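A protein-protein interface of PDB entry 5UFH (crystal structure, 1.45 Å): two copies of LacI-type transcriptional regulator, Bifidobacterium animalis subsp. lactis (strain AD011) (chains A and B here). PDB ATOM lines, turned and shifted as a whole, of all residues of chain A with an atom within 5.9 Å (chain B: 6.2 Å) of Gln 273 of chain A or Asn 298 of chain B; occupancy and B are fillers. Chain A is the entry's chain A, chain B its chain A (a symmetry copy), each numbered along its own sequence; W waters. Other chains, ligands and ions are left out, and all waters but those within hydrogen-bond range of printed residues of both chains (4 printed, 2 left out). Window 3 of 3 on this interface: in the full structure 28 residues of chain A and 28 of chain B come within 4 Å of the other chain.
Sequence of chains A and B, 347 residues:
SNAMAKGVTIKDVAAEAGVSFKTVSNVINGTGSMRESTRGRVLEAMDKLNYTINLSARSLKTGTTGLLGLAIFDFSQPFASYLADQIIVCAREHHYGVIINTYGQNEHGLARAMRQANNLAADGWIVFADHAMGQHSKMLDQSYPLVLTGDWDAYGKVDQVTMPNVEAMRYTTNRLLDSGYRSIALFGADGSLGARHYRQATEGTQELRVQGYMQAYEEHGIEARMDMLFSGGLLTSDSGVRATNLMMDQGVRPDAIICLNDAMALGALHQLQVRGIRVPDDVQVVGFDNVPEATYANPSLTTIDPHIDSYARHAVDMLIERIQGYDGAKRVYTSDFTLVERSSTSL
Among the printed residues, pairs that only touch across the chains: Asn 298 of chain A with Leu 269 of chain B and Leu 269 of chain A with Asn 298 of chain B.
Of the printed residues of chain B, Leu 269 of chain A touches Asn 298. Of the printed residues of chain B, His 270 of chain A touches Tyr 296 (3.3 Å), Ala 297 (3.1 Å) and Asn 298 (2.8 Å). Gln 273 of chain A touches one residue of chain B. Pro 299 of chain A touches none of the printed residues of chain B. Printed residues of chain A within 4 Å of Tyr 296 of chain B: His 270 (3.3 Å). Of the printed residues of chain A, Asn 298 of chain B touches Leu 269 (3.9 Å), His 270 (2.8 Å), Gln 273 (3.0 Å) and Asn 298 (3.1 Å). Pro 299 of chain B touches none of the printed residues of chain A. The nearest printed residue of chain B that does not touch His 270 of chain A is Ser 300 of chain B (4.1 Å).
Water W4 lies within hydrogen-bond range of the backbone carbonyl oxygen of Leu 266 of chain A (2.7 Å), the backbone carbonyl oxygen of Tyr 296 of chain B (2.8 Å) and the side-chain amide nitrogen of Asn 298 of chain B (3.1 Å). Water W2 bridges the backbone NH of Asn 298 of chain A and the side-chain amide nitrogen of Asn 298 of chain B. Water W3 lies within hydrogen-bond range of N of Asn 298 of chain B (3.0 Å) and ND2 of Asn 298 of chain A (3.1 Å). Water W1 bridges a ring nitrogen (NE2) of His 270 of chain A (3.3 Å) and the side-chain hydroxyl of Ser 300 of chain B (3.4 Å).
Leu 269 of chain A touches Asn 298 of chain B, and with the chains exchanged Asn 298 of chain A touches Leu 269 of chain B. Gln 273 of chain A touches Asn 298 of chain B, and with the chains exchanged Asn 298 of chain A touches Gln 273 of chain B. Asn 298 of chain B touches its own counterpart, Asn 298 of chain A. Of the 8 pairs that touch across the chains among the printed residues, 5 have their exchanged pair printed and touching as well.
Of the 8 printed residues of chain B, 5 touch a printed residue of chain A. Of the 15 printed residues of chain A, 4 touch a printed residue of chain B. Printed residues of chain A that touch a printed residue of chain B: Leu 269, His 270, Gln 273 and Asn 298. Among the printed residues, 8 pairs touch across the chains.
ND1 of His 270 of chain A lies within hydrogen-bond range of O of Tyr 296 of chain B, 3.3 Å away. The backbone carbonyl oxygen (O) of Ala 297 of chain B is in hydrogen-bond range of a ring nitrogen (ND1) of His 270 of chain A. ND1 of His 270 of chain A lies within hydrogen-bond range of OD1 of Asn 298 of chain B, at 2.8 Å. The side-chain amide nitrogen (NE2) of Gln 273 of chain A lies within hydrogen-bond range of the side-chain amide oxygen (OD1) of Asn 298 of chain B (3.0 Å). The side-chain amide oxygen (OD1) of Asn 298 of chain A lies within hydrogen-bond range of the side-chain amide nitrogen (NE2) of Gln 273 of chain B (3.0 Å). The backbone carbonyl oxygen of Asn 298 of chain A lies within hydrogen-bond range of the side-chain amide nitrogen of Asn 298 of chain B (3.1 Å).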
ATOM      1  N   LEU A 266     -27.153  26.374  -3.801  1.00  0.00           N
ATOM      2  CA  LEU A 266     -26.064  26.705  -2.894  1.00  0.00           C
ATOM      3  C   LEU A 266     -25.320  25.436  -2.503  1.00  0.00           C
ATOM      4  O   LEU A 266     -24.087  25.438  -2.372  1.00  0.00           O
ATOM      5  CB  LEU A 266     -26.652  27.452  -1.688  1.00  0.00           C
ATOM      6  CG  LEU A 266     -27.268  28.787  -2.127  1.00  0.00           C
ATOM      7  CD1 LEU A 266     -28.211  29.353  -1.031  1.00  0.00           C
ATOM      8  CD2 LEU A 266     -26.191  29.776  -2.496  1.00  0.00           C
ATOM      9  N   ALA A 268     -25.126  22.727  -4.424  1.00  0.00           N
ATOM     10  CA  ALA A 268     -24.410  22.354  -5.640  1.00  0.00           C
ATOM     11  C   ALA A 268     -23.154  23.194  -5.841  1.00  0.00           C
ATOM     12  O   ALA A 268     -22.098  22.644  -6.196  1.00  0.00           O
ATOM     13  CB  ALA A 268     -25.333  22.387  -6.862  1.00  0.00           C
ATOM     14  N   LEU A 269     -23.237  24.525  -5.628  1.00  0.00           N
ATOM     15  CA  LEU A 269     -22.021  25.345  -5.755  1.00  0.00           C
ATOM     16  C   LEU A 269     -20.916  24.830  -4.846  1.00  0.00           C
ATOM     17  O   LEU A 269     -19.740  24.761  -5.242  1.00  0.00           O
ATOM     18  CB  LEU A 269     -22.302  26.813  -5.393  1.00  0.00           C
ATOM     19  CG  LEU A 269     -23.151  27.585  -6.382  1.00  0.00           C
ATOM     20  CD1 LEU A 269     -23.309  28.987  -5.841  1.00  0.00           C
ATOM     21  CD2 LEU A 269     -22.482  27.623  -7.778  1.00  0.00           C
ATOM     22  N   HIS A 270     -21.283  24.418  -3.634  1.00  0.00           N
ATOM     23  CA  HIS A 270     -20.296  23.887  -2.718  1.00  0.00           C
ATOM     24  C   HIS A 270     -19.732  22.559  -3.202  1.00  0.00           C
ATOM     25  O   HIS A 270     -18.510  22.375  -3.258  1.00  0.00           O
ATOM     26  CB  HIS A 270     -20.952  23.703  -1.350  1.00  0.00           C
ATOM     27  CG  HIS A 270     -19.998  23.218  -0.331  1.00  0.00           C
ATOM     28  ND1 HIS A 270     -18.959  24.001   0.144  1.00  0.00           N
ATOM     29  CD2 HIS A 270     -19.843  22.000   0.243  1.00  0.00           C
ATOM     30  CE1 HIS A 270     -18.231  23.296   0.987  1.00  0.00           C
ATOM     31  NE2 HIS A 270     -18.736  22.075   1.055  1.00  0.00           N
ATOM     32  N   GLN A 271     -20.606  21.612  -3.568  1.00  0.00           N
ATOM     33  CA  GLN A 271     -20.098  20.273  -3.856  1.00  0.00           C
ATOM     34  C   GLN A 271     -19.359  20.241  -5.185  1.00  0.00           C
ATOM     35  O   GLN A 271     -18.366  19.513  -5.330  1.00  0.00           O
ATOM     36  CB  GLN A 271     -21.249  19.241  -3.784  1.00  0.00           C
ATOM     37  CG  GLN A 271     -20.781  17.779  -3.897  1.00  0.00           C
ATOM     38  CD  GLN A 271     -19.877  17.364  -2.745  1.00  0.00           C
ATOM     39  OE1 GLN A 271     -19.694  18.105  -1.768  1.00  0.00           O
ATOM     40  NE2 GLN A 271     -19.366  16.156  -2.825  1.00  0.00           N
ATOM     41  N   LEU A 272     -19.786  21.059  -6.154  1.00  0.00           N
ATOM     42  CA  LEU A 272     -19.033  21.188  -7.405  1.00  0.00           C
ATOM     43  C   LEU A 272     -17.612  21.657  -7.128  1.00  0.00           C
ATOM     44  O   LEU A 272     -16.640  21.055  -7.603  1.00  0.00           O
ATOM     45  CB  LEU A 272     -19.729  22.139  -8.381  1.00  0.00           C
ATOM     46  CG  LEU A 272     -21.036  21.628  -8.964  1.00  0.00           C
ATOM     47  CD1 LEU A 272     -21.812  22.801  -9.584  1.00  0.00           C
ATOM     48  CD2 LEU A 272     -20.759  20.528 -10.042  1.00  0.00           C
ATOM     49  N   GLN A 273     -17.472  22.707  -6.298  1.00  0.00           N
ATOM     50  CA  GLN A 273     -16.144  23.251  -6.018  1.00  0.00           C
ATOM     51  C   GLN A 273     -15.298  22.254  -5.249  1.00  0.00           C
ATOM     52  O   GLN A 273     -14.088  22.121  -5.507  1.00  0.00           O
ATOM     53  CB  GLN A 273     -16.283  24.562  -5.225  1.00  0.00           C
ATOM     54  CG  GLN A 273     -15.015  25.159  -4.617  1.00  0.00           C
ATOM     55  CD  GLN A 273     -14.705  24.644  -3.204  1.00  0.00           C
ATOM     56  OE1 GLN A 273     -13.707  23.963  -3.013  1.00  0.00           O
ATOM     57  NE2 GLN A 273     -15.557  24.983  -2.212  1.00  0.00           N
ATOM     58  N   VAL A 274     -15.911  21.540  -4.298  1.00  0.00           N
ATOM     59  CA  VAL A 274     -15.190  20.539  -3.511  1.00  0.00           C
ATOM     60  C   VAL A 274     -14.626  19.439  -4.406  1.00  0.00           C
ATOM     61  O   VAL A 274     -13.520  18.929  -4.178  1.00  0.00           O
ATOM     62  CB  VAL A 274     -16.124  19.966  -2.430  1.00  0.00           C
ATOM     63  CG1 VAL A 274     -15.597  18.625  -1.870  1.00  0.00           C
ATOM     64  CG2 VAL A 274     -16.297  21.002  -1.326  1.00  0.00           C
ATOM     65  N   ARG A 275     -15.370  19.067  -5.454  1.00  0.00           N
ATOM     66  CA  ARG A 275     -14.957  18.011  -6.362  1.00  0.00           C
ATOM     67  C   ARG A 275     -14.235  18.551  -7.609  1.00  0.00           C
ATOM     68  O   ARG A 275     -14.111  17.835  -8.610  1.00  0.00           O
ATOM     69  CB  ARG A 275     -16.162  17.125  -6.723  1.00  0.00           C
ATOM     70  CG  ARG A 275     -16.551  16.170  -5.586  1.00  0.00           C
ATOM     71  CD  ARG A 275     -17.657  15.174  -5.902  1.00  0.00           C
ATOM     72  NE  ARG A 275     -17.246  14.193  -6.909  1.00  0.00           N
ATOM     73  CZ  ARG A 275     -17.989  13.159  -7.290  1.00  0.00           C
ATOM     74  NH1 ARG A 275     -19.179  12.947  -6.719  1.00  0.00           N
ATOM     75  NH2 ARG A 275     -17.549  12.328  -8.237  1.00  0.00           N
ATOM     76  N   GLY A 276     -13.772  19.802  -7.575  1.00  0.00           N
ATOM     77  CA  GLY A 276     -12.862  20.297  -8.596  1.00  0.00           C
ATOM     78  C   GLY A 276     -13.509  20.884  -9.825  1.00  0.00           C
ATOM     79  O   GLY A 276     -12.826  21.072 -10.832  1.00  0.00           O
ATOM     80  N   ILE A 277     -14.798  21.205  -9.780  1.00  0.00           N
ATOM     81  CA  ILE A 277     -15.508  21.765 -10.934  1.00  0.00           C
ATOM     82  C   ILE A 277     -15.632  23.261 -10.724  1.00  0.00           C
ATOM     83  O   ILE A 277     -16.133  23.708  -9.682  1.00  0.00           O
ATOM     84  CB  ILE A 277     -16.884  21.112 -11.131  1.00  0.00           C
ATOM     85  CG1 ILE A 277     -16.765  19.587 -11.248  1.00  0.00           C
ATOM     86  CG2 ILE A 277     -17.621  21.747 -12.315  1.00  0.00           C
ATOM     87  CD1 ILE A 277     -15.814  19.086 -12.352  1.00  0.00           C
ATOM     88  N   ARG A 278     -15.182  24.038 -11.712  1.00  0.00           N
ATOM     89  CA  ARG A 278     -15.216  25.485 -11.625  1.00  0.00           C
ATOM     90  C   ARG A 278     -16.563  25.983 -12.119  1.00  0.00           C
ATOM     91  O   ARG A 278     -17.056  25.554 -13.175  1.00  0.00           O
ATOM     92  CB  ARG A 278     -14.101  26.084 -12.489  1.00  0.00           C
ATOM     93  CG  ARG A 278     -12.720  25.720 -11.972  1.00  0.00           C
ATOM     94  N   VAL A 279     -17.148  26.893 -11.350  1.00  0.00           N
ATOM     95  CA  VAL A 279     -18.370  27.601 -11.702  1.00  0.00           C
ATOM     96  C   VAL A 279     -18.022  29.076 -11.841  1.00  0.00           C
ATOM     97  O   VAL A 279     -17.530  29.679 -10.876  1.00  0.00           O
ATOM     98  CB  VAL A 279     -19.435  27.407 -10.615  1.00  0.00           C
ATOM     99  CG1 VAL A 279     -20.682  28.157 -11.034  1.00  0.00           C
ATOM    100  CG2 VAL A 279     -19.696  25.933 -10.459  1.00  0.00           C
ATOM    101  N   ASN A 298     -20.471  32.311  -3.237  1.00  0.00           N
ATOM    102  CA  ASN A 298     -19.175  32.441  -3.896  1.00  0.00           C
ATOM    103  C   ASN A 298     -19.055  31.249  -4.827  1.00  0.00           C
ATOM    104  O   ASN A 298     -18.795  30.124  -4.368  1.00  0.00           O
ATOM    105  CB  ASN A 298     -18.021  32.483  -2.899  1.00  0.00           C
ATOM    106  CG  ASN A 298     -18.188  33.637  -1.892  1.00  0.00           C
ATOM    107  OD1 ASN A 298     -18.341  34.795  -2.271  1.00  0.00           O
ATOM    108  ND2 ASN A 298     -18.183  33.317  -0.602  1.00  0.00           N
ATOM    109  N   PRO A 299     -19.277  31.427  -6.126  1.00  0.00           N
ATOM    110  CA  PRO A 299     -19.609  32.683  -6.817  1.00  0.00           C
ATOM    111  C   PRO A 299     -21.056  33.054  -6.549  1.00  0.00           C
ATOM    112  O   PRO A 299     -21.911  32.190  -6.277  1.00  0.00           O
ATOM    113  CB  PRO A 299     -19.460  32.306  -8.300  1.00  0.00           C
ATOM    114  CG  PRO A 299     -19.770  30.830  -8.351  1.00  0.00           C
ATOM    115  CD  PRO A 299     -19.269  30.260  -7.025  1.00  0.00           C
ATOM    116  N   LEU B 269     -17.034  36.604   4.002  1.00  0.00           N
ATOM    117  CA  LEU B 269     -16.391  35.710   3.025  1.00  0.00           C
ATOM    118  C   LEU B 269     -16.630  36.190   1.602  1.00  0.00           C
ATOM    119  O   LEU B 269     -15.719  36.175   0.759  1.00  0.00           O
ATOM    120  CB  LEU B 269     -16.930  34.275   3.150  1.00  0.00           C
ATOM    121  CG  LEU B 269     -16.514  33.520   4.395  1.00  0.00           C
ATOM    122  CD1 LEU B 269     -17.147  32.150   4.324  1.00  0.00           C
ATOM    123  CD2 LEU B 269     -14.973  33.393   4.479  1.00  0.00           C
ATOM    124  N   GLN B 273     -13.589  38.052  -0.797  1.00  0.00           N
ATOM    125  CA  GLN B 273     -13.233  37.440  -2.076  1.00  0.00           C
ATOM    126  C   GLN B 273     -13.444  38.411  -3.222  1.00  0.00           C
ATOM    127  O   GLN B 273     -12.633  38.463  -4.164  1.00  0.00           O
ATOM    128  CB  GLN B 273     -14.072  36.169  -2.288  1.00  0.00           C
ATOM    129  CG  GLN B 273     -14.035  35.519  -3.670  1.00  0.00           C
ATOM    130  CD  GLN B 273     -15.096  36.064  -4.638  1.00  0.00           C
ATOM    131  OE1 GLN B 273     -14.747  36.690  -5.629  1.00  0.00           O
ATOM    132  NE2 GLN B 273     -16.392  35.812  -4.354  1.00  0.00           N
ATOM    133  N   TYR B 296     -21.933  24.842   3.865  1.00  0.00           N
ATOM    134  CA  TYR B 296     -21.955  24.912   2.408  1.00  0.00           C
ATOM    135  C   TYR B 296     -21.281  26.152   1.865  1.00  0.00           C
ATOM    136  O   TYR B 296     -21.259  26.322   0.660  1.00  0.00           O
ATOM    137  CB  TYR B 296     -23.399  24.843   1.852  1.00  0.00           C
ATOM    138  CG  TYR B 296     -24.174  23.705   2.439  1.00  0.00           C
ATOM    139  CD1 TYR B 296     -23.999  22.401   1.963  1.00  0.00           C
ATOM    140  CD2 TYR B 296     -25.063  23.917   3.482  1.00  0.00           C
ATOM    141  CE1 TYR B 296     -24.693  21.334   2.517  1.00  0.00           C
ATOM    142  CE2 TYR B 296     -25.742  22.866   4.047  1.00  0.00           C
ATOM    143  CZ  TYR B 296     -25.559  21.594   3.561  1.00  0.00           C
ATOM    144  OH  TYR B 296     -26.239  20.553   4.122  1.00  0.00           O
ATOM    145  N   ALA B 297     -20.729  27.002   2.735  1.00  0.00           N
ATOM    146  CA  ALA B 297     -20.045  28.191   2.267  1.00  0.00           C
ATOM    147  C   ALA B 297     -18.796  27.798   1.470  1.00  0.00           C
ATOM    148  O   ALA B 297     -18.303  26.660   1.549  1.00  0.00           O
ATOM    149  CB  ALA B 297     -19.665  29.078   3.478  1.00  0.00           C
ATOM    150  N   ASN B 298     -18.274  28.757   0.705  1.00  0.00           N
ATOM    151  CA  ASN B 298     -17.085  28.528  -0.111  1.00  0.00           C
ATOM    152  C   ASN B 298     -16.141  29.676   0.188  1.00  0.00           C
ATOM    153  O   ASN B 298     -16.353  30.799  -0.300  1.00  0.00           O
ATOM    154  CB  ASN B 298     -17.412  28.451  -1.599  1.00  0.00           C
ATOM    155  CG  ASN B 298     -18.443  27.347  -1.895  1.00  0.00           C
ATOM    156  OD1 ASN B 298     -18.253  26.187  -1.539  1.00  0.00           O
ATOM    157  ND2 ASN B 298     -19.553  27.711  -2.529  1.00  0.00           N
ATOM    158  N   PRO B 299     -15.118  29.466   1.011  1.00  0.00           N
ATOM    159  CA  PRO B 299     -14.746  28.208   1.679  1.00  0.00           C
ATOM    160  C   PRO B 299     -15.694  27.934   2.832  1.00  0.00           C
ATOM    161  O   PRO B 299     -16.288  28.857   3.420  1.00  0.00           O
ATOM    162  CB  PRO B 299     -13.352  28.523   2.246  1.00  0.00           C
ATOM    163  CG  PRO B 299     -13.367  30.013   2.490  1.00  0.00           C
ATOM    164  CD  PRO B 299     -14.258  30.598   1.395  1.00  0.00           C
ATOM    165  N   SER B 300     -15.802  26.650   3.188  1.00  0.00           N
ATOM    166  CA  SER B 300     -16.659  26.289   4.313  1.00  0.00           C
ATOM    167  C   SER B 300     -16.182  26.981   5.590  1.00  0.00           C
ATOM    168  O   SER B 300     -14.992  27.271   5.760  1.00  0.00           O
ATOM    169  CB  SER B 300     -16.659  24.779   4.504  1.00  0.00           C
ATOM    170  OG  SER B 300     -15.330  24.274   4.642  1.00  0.00           O
ATOM    171  N   LEU B 301     -17.146  27.344   6.445  1.00  0.00           N
ATOM    172  CA  LEU B 301     -16.919  28.342   7.486  1.00  0.00           C
ATOM    173  C   LEU B 301     -16.582  27.692   8.831  1.00  0.00           C
ATOM    174  O   LEU B 301     -17.402  26.956   9.395  1.00  0.00           O
ATOM    175  CB  LEU B 301     -18.127  29.257   7.604  1.00  0.00           C
ATOM    176  CG  LEU B 301     -18.048  30.270   8.759  1.00  0.00           C
ATOM    177  CD1 LEU B 301     -16.978  31.297   8.516  1.00  0.00           C
ATOM    178  CD2 LEU B 301     -19.430  30.909   8.848  1.00  0.00           C
HETATM  179  O   HOH W   1     -15.854  21.673   2.522  1.00  0.00           O
HETATM  180  O   HOH W   2     -21.342  30.046  -1.511  1.00  0.00           O
HETATM  181  O   HOH W   3     -20.068  31.130   0.561  1.00  0.00           O
HETATM  182  O   HOH W   4     -22.474  27.490  -1.533  1.00  0.00           O
